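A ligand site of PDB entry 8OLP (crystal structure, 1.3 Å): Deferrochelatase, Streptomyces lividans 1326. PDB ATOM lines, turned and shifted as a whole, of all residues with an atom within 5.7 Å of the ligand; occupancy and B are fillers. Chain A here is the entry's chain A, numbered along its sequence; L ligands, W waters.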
ATOM      1  N   ASN A 233     -25.232  25.071 -17.501  1.00  0.00           N
ATOM      2  CA  ASN A 233     -26.146  26.078 -16.981  1.00  0.00           C
ATOM      3  C   ASN A 233     -25.462  27.426 -16.866  1.00  0.00           C
ATOM      4  O   ASN A 233     -24.256  27.593 -17.189  1.00  0.00           O
ATOM      5  CB  ASN A 233     -26.795  25.559 -15.678  1.00  0.00           C
ATOM      6  CG  ASN A 233     -25.764  25.309 -14.603  1.00  0.00           C
ATOM      7  OD1 ASN A 233     -24.832  26.107 -14.440  1.00  0.00           O
ATOM      8  ND2 ASN A 233     -25.981  24.221 -13.885  1.00  0.00           N
ATOM      9  N   LEU A 235     -24.542  29.007 -14.299  1.00  0.00           N
ATOM     10  CA  LEU A 235     -23.451  29.015 -13.347  1.00  0.00           C
ATOM     11  C   LEU A 235     -22.164  28.459 -13.915  1.00  0.00           C
ATOM     12  O   LEU A 235     -21.130  28.459 -13.234  1.00  0.00           O
ATOM     13  CB  LEU A 235     -23.831  28.278 -12.066  1.00  0.00           C
ATOM     14  CG  LEU A 235     -25.105  28.780 -11.378  1.00  0.00           C
ATOM     15  CD1 LEU A 235     -25.322  28.001 -10.105  1.00  0.00           C
ATOM     16  CD2 LEU A 235     -25.080  30.286 -11.148  1.00  0.00           C
ATOM     17  N   PHE A 237     -21.520  25.367 -14.975  1.00  0.00           N
ATOM     18  CA  PHE A 237     -21.284  23.956 -14.738  1.00  0.00           C
ATOM     19  C   PHE A 237     -22.107  23.101 -15.701  1.00  0.00           C
ATOM     20  O   PHE A 237     -23.273  23.375 -16.005  1.00  0.00           O
ATOM     21  CB  PHE A 237     -21.650  23.565 -13.311  1.00  0.00           C
ATOM     22  CG  PHE A 237     -20.566  23.893 -12.323  1.00  0.00           C
ATOM     23  CD1 PHE A 237     -20.303  25.211 -11.958  1.00  0.00           C
ATOM     24  CD2 PHE A 237     -19.759  22.894 -11.753  1.00  0.00           C
ATOM     25  CE1 PHE A 237     -19.318  25.505 -11.032  1.00  0.00           C
ATOM     26  CE2 PHE A 237     -18.760  23.204 -10.820  1.00  0.00           C
ATOM     27  CZ  PHE A 237     -18.523  24.521 -10.510  1.00  0.00           C
ATOM     28  N   LYS A 238     -21.521  21.967 -16.121  1.00  0.00           N
ATOM     29  CA  LYS A 238     -22.261  20.942 -16.811  1.00  0.00           C
ATOM     30  C   LYS A 238     -23.392  20.439 -15.936  1.00  0.00           C
ATOM     31  O   LYS A 238     -23.205  20.283 -14.703  1.00  0.00           O
ATOM     32  CB  LYS A 238     -21.335  19.739 -17.110  1.00  0.00           C
ATOM     33  CG  LYS A 238     -20.221  20.017 -18.113  1.00  0.00           C
ATOM     34  CD  LYS A 238     -19.333  18.811 -18.251  1.00  0.00           C
ATOM     35  CE  LYS A 238     -18.229  19.020 -19.260  1.00  0.00           C
ATOM     36  NZ  LYS A 238     -17.347  17.855 -19.311  1.00  0.00           N
ATOM     37  N   ASP A 239     -24.548  20.210 -16.560  1.00  0.00           N
ATOM     38  CA  ASP A 239     -25.763  19.899 -15.824  1.00  0.00           C
ATOM     39  C   ASP A 239     -26.479  18.817 -16.603  1.00  0.00           C
ATOM     40  O   ASP A 239     -26.889  19.033 -17.767  1.00  0.00           O
ATOM     41  CB  ASP A 239     -26.637  21.163 -15.663  1.00  0.00           C
ATOM     42  CG  ASP A 239     -27.661  21.142 -14.539  1.00  0.00           C
ATOM     43  OD1 ASP A 239     -28.025  20.018 -14.044  1.00  0.00           O
ATOM     44  OD2 ASP A 239     -28.066  22.252 -14.156  1.00  0.00           O
ATOM     45  N   GLY A 240     -26.501  17.585 -16.061  1.00  0.00           N
ATOM     46  CA  GLY A 240     -27.148  16.488 -16.694  1.00  0.00           C
ATOM     47  C   GLY A 240     -26.269  15.223 -16.796  1.00  0.00           C
ATOM     48  O   GLY A 240     -26.711  14.225 -17.286  1.00  0.00           O
ATOM     49  N   THR A 241     -25.055  15.234 -16.201  1.00  0.00           N
ATOM     50  CA  THR A 241     -24.146  14.106 -16.246  1.00  0.00           C
ATOM     51  C   THR A 241     -24.829  12.811 -15.753  1.00  0.00           C
ATOM     52  O   THR A 241     -24.803  11.799 -16.434  1.00  0.00           O
ATOM     53  CB  THR A 241     -22.863  14.394 -15.501  1.00  0.00           C
ATOM     54  OG1 THR A 241     -22.258  15.574 -16.005  1.00  0.00           O
ATOM     55  CG2 THR A 241     -21.914  13.199 -15.536  1.00  0.00           C
ATOM     56  N   ARG A 242     -25.301  12.840 -14.532  1.00  0.00           N
ATOM     57  CA  ARG A 242     -25.901  11.648 -13.916  1.00  0.00           C
ATOM     58  C   ARG A 242     -27.431  11.859 -13.845  1.00  0.00           C
ATOM     59  O   ARG A 242     -27.991  12.328 -12.868  1.00  0.00           O
ATOM     60  CB  ARG A 242     -25.299  11.371 -12.527  1.00  0.00           C
ATOM     61  CG  ARG A 242     -24.008  10.586 -12.558  1.00  0.00           C
ATOM     62  CD  ARG A 242     -23.386  10.322 -11.211  1.00  0.00           C
ATOM     63  NE  ARG A 242     -24.360   9.892 -10.248  1.00  0.00           N
ATOM     64  CZ  ARG A 242     -25.094   8.781 -10.299  1.00  0.00           C
ATOM     65  NH1 ARG A 242     -26.266   8.737  -9.676  1.00  0.00           N
ATOM     66  NH2 ARG A 242     -24.683   7.736 -11.025  1.00  0.00           N
ATOM     67  N   ASN A 243     -28.060  11.481 -14.950  1.00  0.00           N
ATOM     68  CA  ASN A 243     -29.497  11.623 -15.143  1.00  0.00           C
ATOM     69  C   ASN A 243     -30.050  10.256 -15.486  1.00  0.00           C
ATOM     70  O   ASN A 243     -29.679   9.275 -14.834  1.00  0.00           O
ATOM     71  CB  ASN A 243     -29.789  12.709 -16.174  1.00  0.00           C
ATOM     72  CG  ASN A 243     -31.223  13.219 -16.111  1.00  0.00           C
ATOM     73  OD1 ASN A 243     -31.762  13.452 -15.036  1.00  0.00           O
ATOM     74  ND2 ASN A 243     -31.829  13.406 -17.269  1.00  0.00           N
ATOM     75  N   ILE A 278     -36.271  28.730 -11.112  1.00  0.00           N
ATOM     76  CA  ILE A 278     -35.245  28.964 -10.112  1.00  0.00           C
ATOM     77  C   ILE A 278     -34.346  30.130 -10.513  1.00  0.00           C
ATOM     78  O   ILE A 278     -33.599  30.045 -11.473  1.00  0.00           O
ATOM     79  CB  ILE A 278     -34.391  27.706  -9.799  1.00  0.00           C
ATOM     80  CG1 ILE A 278     -35.243  26.487  -9.513  1.00  0.00           C
ATOM     81  CG2 ILE A 278     -33.392  27.997  -8.674  1.00  0.00           C
ATOM     82  CD1 ILE A 278     -34.516  25.166  -9.298  1.00  0.00           C
ATOM     83  N   MET A 280     -31.271  32.588 -10.333  1.00  0.00           N
ATOM     84  CA  MET A 280     -29.879  32.538  -9.893  1.00  0.00           C
ATOM     85  C   MET A 280     -29.394  33.912  -9.461  1.00  0.00           C
ATOM     86  O   MET A 280     -29.608  34.897 -10.151  1.00  0.00           O
ATOM     87  CB  MET A 280     -29.018  32.087 -11.082  1.00  0.00           C
ATOM     88  CG  MET A 280     -29.173  30.604 -11.345  1.00  0.00           C
ATOM     89  SD  MET A 280     -28.482  30.135 -12.946  1.00  0.00           S
ATOM     90  CE  MET A 280     -28.547  28.338 -12.789  1.00  0.00           C
ATOM     91  N   PHE A 297     -20.841  22.378  -5.647  1.00  0.00           N
ATOM     92  CA  PHE A 297     -21.375  21.255  -6.402  1.00  0.00           C
ATOM     93  C   PHE A 297     -20.811  19.889  -6.006  1.00  0.00           C
ATOM     94  O   PHE A 297     -21.510  18.907  -6.006  1.00  0.00           O
ATOM     95  CB  PHE A 297     -21.239  21.490  -7.896  1.00  0.00           C
ATOM     96  CG  PHE A 297     -22.265  22.458  -8.362  1.00  0.00           C
ATOM     97  CD1 PHE A 297     -23.614  22.156  -8.290  1.00  0.00           C
ATOM     98  CD2 PHE A 297     -21.902  23.719  -8.805  1.00  0.00           C
ATOM     99  CE1 PHE A 297     -24.588  23.087  -8.668  1.00  0.00           C
ATOM    100  CE2 PHE A 297     -22.856  24.638  -9.208  1.00  0.00           C
ATOM    101  CZ  PHE A 297     -24.190  24.306  -9.157  1.00  0.00           C
ATOM    102  N   ARG A 299     -18.164  18.877  -7.871  1.00  0.00           N
ATOM    103  CA  ARG A 299     -17.488  18.601  -9.119  1.00  0.00           C
ATOM    104  C   ARG A 299     -16.618  19.799  -9.493  1.00  0.00           C
ATOM    105  O   ARG A 299     -16.921  20.925  -9.095  1.00  0.00           O
ATOM    106  CB  ARG A 299     -18.500  18.337 -10.235  1.00  0.00           C
ATOM    107  CG  ARG A 299     -19.249  17.029 -10.121  1.00  0.00           C
ATOM    108  CD  ARG A 299     -20.306  16.853 -11.186  1.00  0.00           C
ATOM    109  NE  ARG A 299     -21.038  15.561 -11.100  1.00  0.00           N
ATOM    110  CZ  ARG A 299     -20.627  14.442 -11.706  1.00  0.00           C
ATOM    111  NH1 ARG A 299     -19.541  14.420 -12.486  1.00  0.00           N
ATOM    112  NH2 ARG A 299     -21.372  13.349 -11.624  1.00  0.00           N
ATOM    113  N   PRO A 316     -19.055   9.379  -8.735  1.00  0.00           N
ATOM    114  CA  PRO A 316     -18.569  10.131  -7.582  1.00  0.00           C
ATOM    115  C   PRO A 316     -18.268   9.271  -6.373  1.00  0.00           C
ATOM    116  O   PRO A 316     -18.836   8.205  -6.199  1.00  0.00           O
ATOM    117  CB  PRO A 316     -19.762  11.050  -7.293  1.00  0.00           C
ATOM    118  CG  PRO A 316     -20.953  10.355  -7.858  1.00  0.00           C
ATOM    119  CD  PRO A 316     -20.432   9.699  -9.126  1.00  0.00           C
ATOM    120  N   HIS A 326     -24.073  20.000  -3.398  1.00  0.00           N
ATOM    121  CA  HIS A 326     -25.289  19.715  -4.155  1.00  0.00           C
ATOM    122  C   HIS A 326     -25.353  18.241  -4.585  1.00  0.00           C
ATOM    123  O   HIS A 326     -26.353  17.511  -4.393  1.00  0.00           O
ATOM    124  CB  HIS A 326     -25.384  20.651  -5.354  1.00  0.00           C
ATOM    125  CG  HIS A 326     -26.633  20.469  -6.146  1.00  0.00           C
ATOM    126  ND1 HIS A 326     -27.870  20.824  -5.691  1.00  0.00           N
ATOM    127  CD2 HIS A 326     -26.800  19.984  -7.393  1.00  0.00           C
ATOM    128  CE1 HIS A 326     -28.738  20.604  -6.687  1.00  0.00           C
ATOM    129  NE2 HIS A 326     -28.108  20.098  -7.748  1.00  0.00           N
ATOM    130  N   VAL A 327     -24.296  17.771  -5.235  1.00  0.00           N
ATOM    131  CA  VAL A 327     -24.298  16.394  -5.735  1.00  0.00           C
ATOM    132  C   VAL A 327     -24.426  15.364  -4.626  1.00  0.00           C
ATOM    133  O   VAL A 327     -25.178  14.403  -4.747  1.00  0.00           O
ATOM    134  CB  VAL A 327     -23.082  16.140  -6.638  1.00  0.00           C
ATOM    135  CG1 VAL A 327     -22.920  14.651  -6.940  1.00  0.00           C
ATOM    136  CG2 VAL A 327     -23.167  16.932  -7.930  1.00  0.00           C
ATOM    137  N   ALA A 330     -28.037  15.459  -3.485  1.00  0.00           N
ATOM    138  CA  ALA A 330     -29.025  15.144  -4.495  1.00  0.00           C
ATOM    139  C   ALA A 330     -28.914  13.691  -4.992  1.00  0.00           C
ATOM    140  O   ALA A 330     -29.848  13.167  -5.604  1.00  0.00           O
ATOM    141  CB  ALA A 330     -28.906  16.044  -5.672  1.00  0.00           C
ATOM    142  N   HIS A 331     -27.798  13.022  -4.701  1.00  0.00           N
ATOM    143  CA  HIS A 331     -27.504  11.724  -5.314  1.00  0.00           C
ATOM    144  C   HIS A 331     -28.521  10.700  -4.826  1.00  0.00           C
ATOM    145  O   HIS A 331     -28.950  10.747  -3.674  1.00  0.00           O
ATOM    146  CB  HIS A 331     -26.104  11.277  -4.899  1.00  0.00           C
ATOM    147  CG  HIS A 331     -25.568  10.102  -5.612  1.00  0.00           C
ATOM    148  ND1 HIS A 331     -25.941   8.781  -5.336  1.00  0.00           N
ATOM    149  CD2 HIS A 331     -24.628  10.053  -6.573  1.00  0.00           C
ATOM    150  CE1 HIS A 331     -25.270   7.986  -6.156  1.00  0.00           C
ATOM    151  NE2 HIS A 331     -24.480   8.723  -6.916  1.00  0.00           N
ATOM    152  N   PRO A 332     -28.940   9.733  -5.672  1.00  0.00           N
ATOM    153  CA  PRO A 332     -29.853   8.702  -5.208  1.00  0.00           C
ATOM    154  C   PRO A 332     -29.434   8.025  -3.905  1.00  0.00           C
ATOM    155  O   PRO A 332     -30.295   7.742  -3.097  1.00  0.00           O
ATOM    156  CB  PRO A 332     -29.895   7.732  -6.365  1.00  0.00           C
ATOM    157  CG  PRO A 332     -29.760   8.645  -7.549  1.00  0.00           C
ATOM    158  CD  PRO A 332     -28.724   9.688  -7.130  1.00  0.00           C
ATOM    159  N   LEU A 340     -34.294  10.911 -10.505  1.00  0.00           N
ATOM    160  CA  LEU A 340     -35.117  11.803 -11.309  1.00  0.00           C
ATOM    161  C   LEU A 340     -34.667  11.728 -12.758  1.00  0.00           C
ATOM    162  O   LEU A 340     -33.486  11.527 -13.022  1.00  0.00           O
ATOM    163  CB  LEU A 340     -34.991  13.248 -10.812  1.00  0.00           C
ATOM    164  CG  LEU A 340     -35.135  13.512  -9.324  1.00  0.00           C
ATOM    165  CD1 LEU A 340     -34.935  14.977  -8.985  1.00  0.00           C
ATOM    166  CD2 LEU A 340     -36.525  13.068  -8.867  1.00  0.00           C
ATOM    167  N   ARG A 342     -34.237  14.678 -15.032  1.00  0.00           N
ATOM    168  CA  ARG A 342     -34.205  16.138 -15.084  1.00  0.00           C
ATOM    169  C   ARG A 342     -34.140  16.570 -16.548  1.00  0.00           C
ATOM    170  O   ARG A 342     -33.463  15.949 -17.343  1.00  0.00           O
ATOM    171  CB  ARG A 342     -32.968  16.676 -14.363  1.00  0.00           C
ATOM    172  CG  ARG A 342     -33.016  16.484 -12.846  1.00  0.00           C
ATOM    173  CD  ARG A 342     -31.701  16.808 -12.144  1.00  0.00           C
ATOM    174  NE  ARG A 342     -30.663  15.854 -12.498  1.00  0.00           N
ATOM    175  CZ  ARG A 342     -29.409  16.133 -12.831  1.00  0.00           C
ATOM    176  NH1 ARG A 342     -28.980  17.387 -12.920  1.00  0.00           N
ATOM    177  NH2 ARG A 342     -28.602  15.120 -13.144  1.00  0.00           N
ATOM    178  N   LEU A 361     -32.789  29.143 -14.016  1.00  0.00           N
ATOM    179  CA  LEU A 361     -32.956  27.833 -14.599  1.00  0.00           C
ATOM    180  C   LEU A 361     -34.391  27.390 -14.360  1.00  0.00           C
ATOM    181  O   LEU A 361     -34.899  27.473 -13.242  1.00  0.00           O
ATOM    182  CB  LEU A 361     -31.934  26.897 -13.921  1.00  0.00           C
ATOM    183  CG  LEU A 361     -31.703  25.566 -14.626  1.00  0.00           C
ATOM    184  CD1 LEU A 361     -30.281  25.055 -14.365  1.00  0.00           C
ATOM    185  CD2 LEU A 361     -32.750  24.555 -14.232  1.00  0.00           C
ATOM    186  N   PHE A 363     -36.295  24.534 -14.064  1.00  0.00           N
ATOM    187  CA  PHE A 363     -36.057  23.162 -13.695  1.00  0.00           C
ATOM    188  C   PHE A 363     -37.293  22.307 -13.982  1.00  0.00           C
ATOM    189  O   PHE A 363     -38.389  22.707 -13.596  1.00  0.00           O
ATOM    190  CB  PHE A 363     -35.677  23.131 -12.215  1.00  0.00           C
ATOM    191  CG  PHE A 363     -35.398  21.744 -11.648  1.00  0.00           C
ATOM    192  CD1 PHE A 363     -36.432  20.969 -11.143  1.00  0.00           C
ATOM    193  CD2 PHE A 363     -34.113  21.231 -11.649  1.00  0.00           C
ATOM    194  CE1 PHE A 363     -36.156  19.699 -10.645  1.00  0.00           C
ATOM    195  CE2 PHE A 363     -33.839  20.003 -11.100  1.00  0.00           C
ATOM    196  CZ  PHE A 363     -34.866  19.206 -10.670  1.00  0.00           C
ATOM    197  N   PHE A 374     -39.138  14.023  -6.660  1.00  0.00           N
ATOM    198  CA  PHE A 374     -38.769  15.394  -6.365  1.00  0.00           C
ATOM    199  C   PHE A 374     -38.857  15.729  -4.878  1.00  0.00           C
ATOM    200  O   PHE A 374     -37.960  16.399  -4.345  1.00  0.00           O
ATOM    201  CB  PHE A 374     -39.625  16.362  -7.186  1.00  0.00           C
ATOM    202  CG  PHE A 374     -39.300  17.801  -6.886  1.00  0.00           C
ATOM    203  CD1 PHE A 374     -38.275  18.436  -7.538  1.00  0.00           C
ATOM    204  CD2 PHE A 374     -39.979  18.536  -5.934  1.00  0.00           C
ATOM    205  CE1 PHE A 374     -37.940  19.739  -7.267  1.00  0.00           C
ATOM    206  CE2 PHE A 374     -39.675  19.862  -5.679  1.00  0.00           C
ATOM    207  CZ  PHE A 374     -38.632  20.462  -6.344  1.00  0.00           C
ATOM    208  N   VAL A 377     -35.987  14.490  -2.567  1.00  0.00           N
ATOM    209  CA  VAL A 377     -34.732  15.056  -2.994  1.00  0.00           C
ATOM    210  C   VAL A 377     -34.668  16.542  -2.617  1.00  0.00           C
ATOM    211  O   VAL A 377     -33.686  17.008  -2.001  1.00  0.00           O
ATOM    212  CB  VAL A 377     -34.436  14.819  -4.481  1.00  0.00           C
ATOM    213  CG1 VAL A 377     -33.127  15.529  -4.899  1.00  0.00           C
ATOM    214  CG2 VAL A 377     -34.303  13.359  -4.843  1.00  0.00           C
ATOM    215  N   GLN A 378     -35.703  17.303  -2.936  1.00  0.00           N
ATOM    216  CA  GLN A 378     -35.714  18.690  -2.571  1.00  0.00           C
ATOM    217  C   GLN A 378     -35.669  18.928  -1.075  1.00  0.00           C
ATOM    218  O   GLN A 378     -35.026  19.853  -0.597  1.00  0.00           O
ATOM    219  CB  GLN A 378     -36.871  19.397  -3.274  1.00  0.00           C
ATOM    220  CG  GLN A 378     -36.996  20.882  -2.885  1.00  0.00           C
ATOM    221  CD  GLN A 378     -35.837  21.760  -3.348  1.00  0.00           C
ATOM    222  OE1 GLN A 378     -35.189  21.537  -4.341  1.00  0.00           O
ATOM    223  NE2 GLN A 378     -35.629  22.833  -2.636  1.00  0.00           N
ATOM    224  N   LEU A 381     -32.240  18.877  -0.033  1.00  0.00           N
ATOM    225  CA  LEU A 381     -31.467  20.065  -0.372  1.00  0.00           C
ATOM    226  C   LEU A 381     -31.730  21.241   0.577  1.00  0.00           C
ATOM    227  O   LEU A 381     -31.198  22.326   0.350  1.00  0.00           O
ATOM    228  CB  LEU A 381     -31.819  20.481  -1.804  1.00  0.00           C
ATOM    229  CG  LEU A 381     -31.507  19.445  -2.890  1.00  0.00           C
ATOM    230  CD1 LEU A 381     -31.837  19.994  -4.266  1.00  0.00           C
ATOM    231  CD2 LEU A 381     -30.103  18.902  -2.837  1.00  0.00           C
ATOM    232  N   LEU A 386     -25.693  25.200  -2.464  1.00  0.00           N
ATOM    233  CA  LEU A 386     -26.243  25.935  -3.609  1.00  0.00           C
ATOM    234  C   LEU A 386     -27.279  26.991  -3.191  1.00  0.00           C
ATOM    235  O   LEU A 386     -27.503  27.956  -3.916  1.00  0.00           O
ATOM    236  CB  LEU A 386     -26.825  24.948  -4.605  1.00  0.00           C
ATOM    237  CG  LEU A 386     -27.391  25.558  -5.886  1.00  0.00           C
ATOM    238  CD1 LEU A 386     -26.372  26.340  -6.707  1.00  0.00           C
ATOM    239  CD2 LEU A 386     -28.081  24.473  -6.696  1.00  0.00           C
ATOM    240  N   ILE A 390     -29.356  30.667  -5.172  1.00  0.00           N
ATOM    241  CA  ILE A 390     -30.590  30.469  -5.931  1.00  0.00           C
ATOM    242  C   ILE A 390     -31.790  30.837  -5.042  1.00  0.00           C
ATOM    243  O   ILE A 390     -31.709  30.935  -3.809  1.00  0.00           O
ATOM    244  CB  ILE A 390     -30.712  29.013  -6.410  1.00  0.00           C
ATOM    245  CG1 ILE A 390     -30.831  28.022  -5.254  1.00  0.00           C
ATOM    246  CG2 ILE A 390     -29.605  28.629  -7.399  1.00  0.00           C
ATOM    247  CD1 ILE A 390     -31.309  26.642  -5.619  1.00  0.00           C
ATOM    248  N   HIS A 392     -36.094  29.665  -5.461  1.00  0.00           N
ATOM    249  CA  HIS A 392     -37.217  29.157  -6.232  1.00  0.00           C
ATOM    250  C   HIS A 392     -38.326  30.218  -6.204  1.00  0.00           C
ATOM    251  O   HIS A 392     -38.797  30.619  -5.143  1.00  0.00           O
ATOM    252  CB  HIS A 392     -37.720  27.846  -5.602  1.00  0.00           C
ATOM    253  CG  HIS A 392     -36.767  26.704  -5.688  1.00  0.00           C
ATOM    254  ND1 HIS A 392     -37.118  25.499  -6.254  1.00  0.00           N
ATOM    255  CD2 HIS A 392     -35.450  26.582  -5.280  1.00  0.00           C
ATOM    256  CE1 HIS A 392     -36.090  24.656  -6.140  1.00  0.00           C
ATOM    257  NE2 HIS A 392     -35.041  25.299  -5.570  1.00  0.00           N
HETATM  258  C1  LIG L   1     -26.713  17.324 -10.315  1.00  0.00           C
HETATM  259  C2  LIG L   1     -26.836  22.129 -10.881  1.00  0.00           C
HETATM  260  C3  LIG L   1     -31.286  22.298  -8.997  1.00  0.00           C
HETATM  261  C4  LIG L   1     -31.204  17.477  -8.494  1.00  0.00           C
HETATM  262  C5  LIG L   1     -26.407  18.619 -10.679  1.00  0.00           C
HETATM  263  C6  LIG L   1     -25.084  18.974 -11.156  1.00  0.00           C
HETATM  264  C7  LIG L   1     -25.112  20.326 -11.326  1.00  0.00           C
HETATM  265  C8  LIG L   1     -26.411  20.828 -10.933  1.00  0.00           C
HETATM  266  C9  LIG L   1     -24.016  21.211 -11.844  1.00  0.00           C
HETATM  267  C10 LIG L   1     -23.919  18.027 -11.482  1.00  0.00           C
HETATM  268  C11 LIG L   1     -23.933  17.305 -12.847  1.00  0.00           C
HETATM  269  C12 LIG L   1     -25.086  16.336 -12.993  1.00  0.00           C
HETATM  270  O1  LIG L   1     -26.230  16.698 -13.474  1.00  0.00           O
HETATM  271  O2  LIG L   1     -24.918  15.103 -12.680  1.00  0.00           O
HETATM  272  C13 LIG L   1     -28.051  22.579 -10.429  1.00  0.00           C
HETATM  273  C14 LIG L   1     -28.485  23.967 -10.464  1.00  0.00           C
HETATM  274  C15 LIG L   1     -29.709  24.035  -9.941  1.00  0.00           C
HETATM  275  C16 LIG L   1     -30.049  22.671  -9.579  1.00  0.00           C
HETATM  276  C17 LIG L   1     -27.662  25.130 -10.971  1.00  0.00           C
HETATM  277  C18 LIG L   1     -30.605  25.177  -9.757  1.00  0.00           C
HETATM  278  C19 LIG L   1     -30.556  26.342 -10.371  1.00  0.00           C
HETATM  279  C20 LIG L   1     -31.655  21.002  -8.658  1.00  0.00           C
HETATM  280  C21 LIG L   1     -32.916  20.622  -8.029  1.00  0.00           C
HETATM  281  C22 LIG L   1     -32.869  19.257  -7.883  1.00  0.00           C
HETATM  282  C23 LIG L   1     -31.642  18.799  -8.426  1.00  0.00           C
HETATM  283  C24 LIG L   1     -33.967  21.634  -7.707  1.00  0.00           C
HETATM  284  C25 LIG L   1     -33.843  18.331  -7.293  1.00  0.00           C
HETATM  285  C26 LIG L   1     -34.738  18.667  -6.434  1.00  0.00           C
HETATM  286  C27 LIG L   1     -30.005  17.055  -9.033  1.00  0.00           C
HETATM  287  C28 LIG L   1     -29.619  15.629  -9.109  1.00  0.00           C
HETATM  288  C29 LIG L   1     -28.402  15.567  -9.591  1.00  0.00           C
HETATM  289  C30 LIG L   1     -27.975  16.960  -9.855  1.00  0.00           C
HETATM  290  C31 LIG L   1     -30.544  14.509  -8.771  1.00  0.00           C
HETATM  291  C32 LIG L   1     -27.602  14.340  -9.858  1.00  0.00           C
HETATM  292  C33 LIG L   1     -26.894  13.792  -8.612  1.00  0.00           C
HETATM  293  C34 LIG L   1     -26.245  12.441  -8.893  1.00  0.00           C
HETATM  294  O3  LIG L   1     -24.978  12.436  -9.049  1.00  0.00           O
HETATM  295  O4  LIG L   1     -26.980  11.403  -8.934  1.00  0.00           O
HETATM  296  N1  LIG L   1     -27.157  19.798 -10.476  1.00  0.00           N
HETATM  297  N2  LIG L   1     -29.031  21.830  -9.918  1.00  0.00           N
HETATM  298  N3  LIG L   1     -30.921  19.840  -8.896  1.00  0.00           N
HETATM  299  N4  LIG L   1     -28.968  17.804  -9.447  1.00  0.00           N
HETATM  300 FE1  LIG L   1     -28.958  19.796  -9.614  1.00  0.00          FE
HETATM  301  O   HOH W   1     -31.838  11.811  -7.158  1.00  0.00           O
HETATM  302  O   HOH W   2     -29.634  19.772 -11.623  1.00  0.00           O
HETATM  303  O   HOH W   3     -28.888  10.902 -10.693  1.00  0.00           O
HETATM  304  O   HOH W   4     -30.403  22.108 -12.829  1.00  0.00           O
HETATM  305  O   HOH W   5     -23.667  14.426 -10.346  1.00  0.00           O
HETATM  306  O   HOH W   6     -31.516  11.455  -9.864  1.00  0.00           O
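Merely in contact with the ligand: Asn 233 (3.5 Å), Leu 235 (3.8 Å), Phe 237 (3.6 Å), Lys 238 (3.1 Å), Asp 239 (3.5 Å), Ile 278 (3.7 Å), Met 280 (3.7 Å), Phe 297 (3.3 Å), Arg 299 (3.8 Å), Val 327 (3.7 Å), Ala 330 (3.5 Å), His 331 (3.5 Å), Pro 332 (3.0 Å), Leu 340 (3.9 Å), Leu 361 (3.8 Å), Phe 363 (3.3 Å), Phe 374 (3.5 Å), Val 377 (3.8 Å), Gln 378 (3.6 Å), Leu 381 (3.8 Å), Leu 386 (3.7 Å) and Ile 390 (3.9 Å).
Hydrophobic or aromatic side chains that line the ligand: Leu 235, Phe 237, Ile 278, Met 280, Phe 297, His 326, Val 327, Ala 330, His 331, Pro 332, Leu 340, Leu 361, Phe 363, Phe 374, Val 377, Leu 381, Leu 386 and Ile 390.
The nearest printed residue that does not touch the ligand is His 392 (4.01 Å).
An iron atom (FE1) of the ligand is bound by a ring nitrogen (NE2) of His 326, at 2.1 Å.
The backbone NH of Gly 240 sits at hydrogen-bond distance from an oxygen (O1) of the ligand, at 2.7 Å.
The backbone NH of Arg 242 sits at hydrogen-bond distance from an oxygen (O2) of the ligand, 2.9 Å away.
The guanidinium group of Arg 242 lies within salt-bridge range of an oxygen (O4) of the ligand, at 2.9 Å.
The guanidinium group (NH2) of Arg 342 lies within salt-bridge range of an oxygen (O1) of the ligand.
O1 of the ligand sits at hydrogen-bond distance from N of Thr 241.
Water W2 lies within hydrogen-bond range of NH1 of Arg 342 (2.8 Å) and OD1 of Asp 239 (2.9 Å).
Water W3 bridges an oxygen (O4) of the ligand (2.6 Å) and the backbone carbonyl oxygen of Arg 242 (2.8 Å).
Water W5 bridges an oxygen (O3) of the ligand (2.7 Å) and the guanidinium group of Arg 299 (2.8 Å).
The guanidinium group of Arg 342 lies within hydrogen-bond range of the backbone carbonyl oxygen of Arg 242.
A ring nitrogen (NE2) of His 331 is in hydrogen-bond range of the guanidinium group (NH1) of Arg 242 (3.3 Å).
O of Phe 297 is in hydrogen-bond range of N of Val 327.
ND2 of Asn 233 is in hydrogen-bond range of OD2 of Asp 239, at 2.9 Å.
OD1 of Asn 233 sits at hydrogen-bond distance from N of Phe 237.
N of Leu 235 lies within hydrogen-bond range of OD1 of Asn 233 (2.9 Å).
The backbone carbonyl oxygen (O) of Ile 278 is in hydrogen-bond range of the backbone NH (N) of Leu 361, 2.8 Å away.
O of Leu 340 lies close to OD1 of Asn 243 (3.3 Å).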
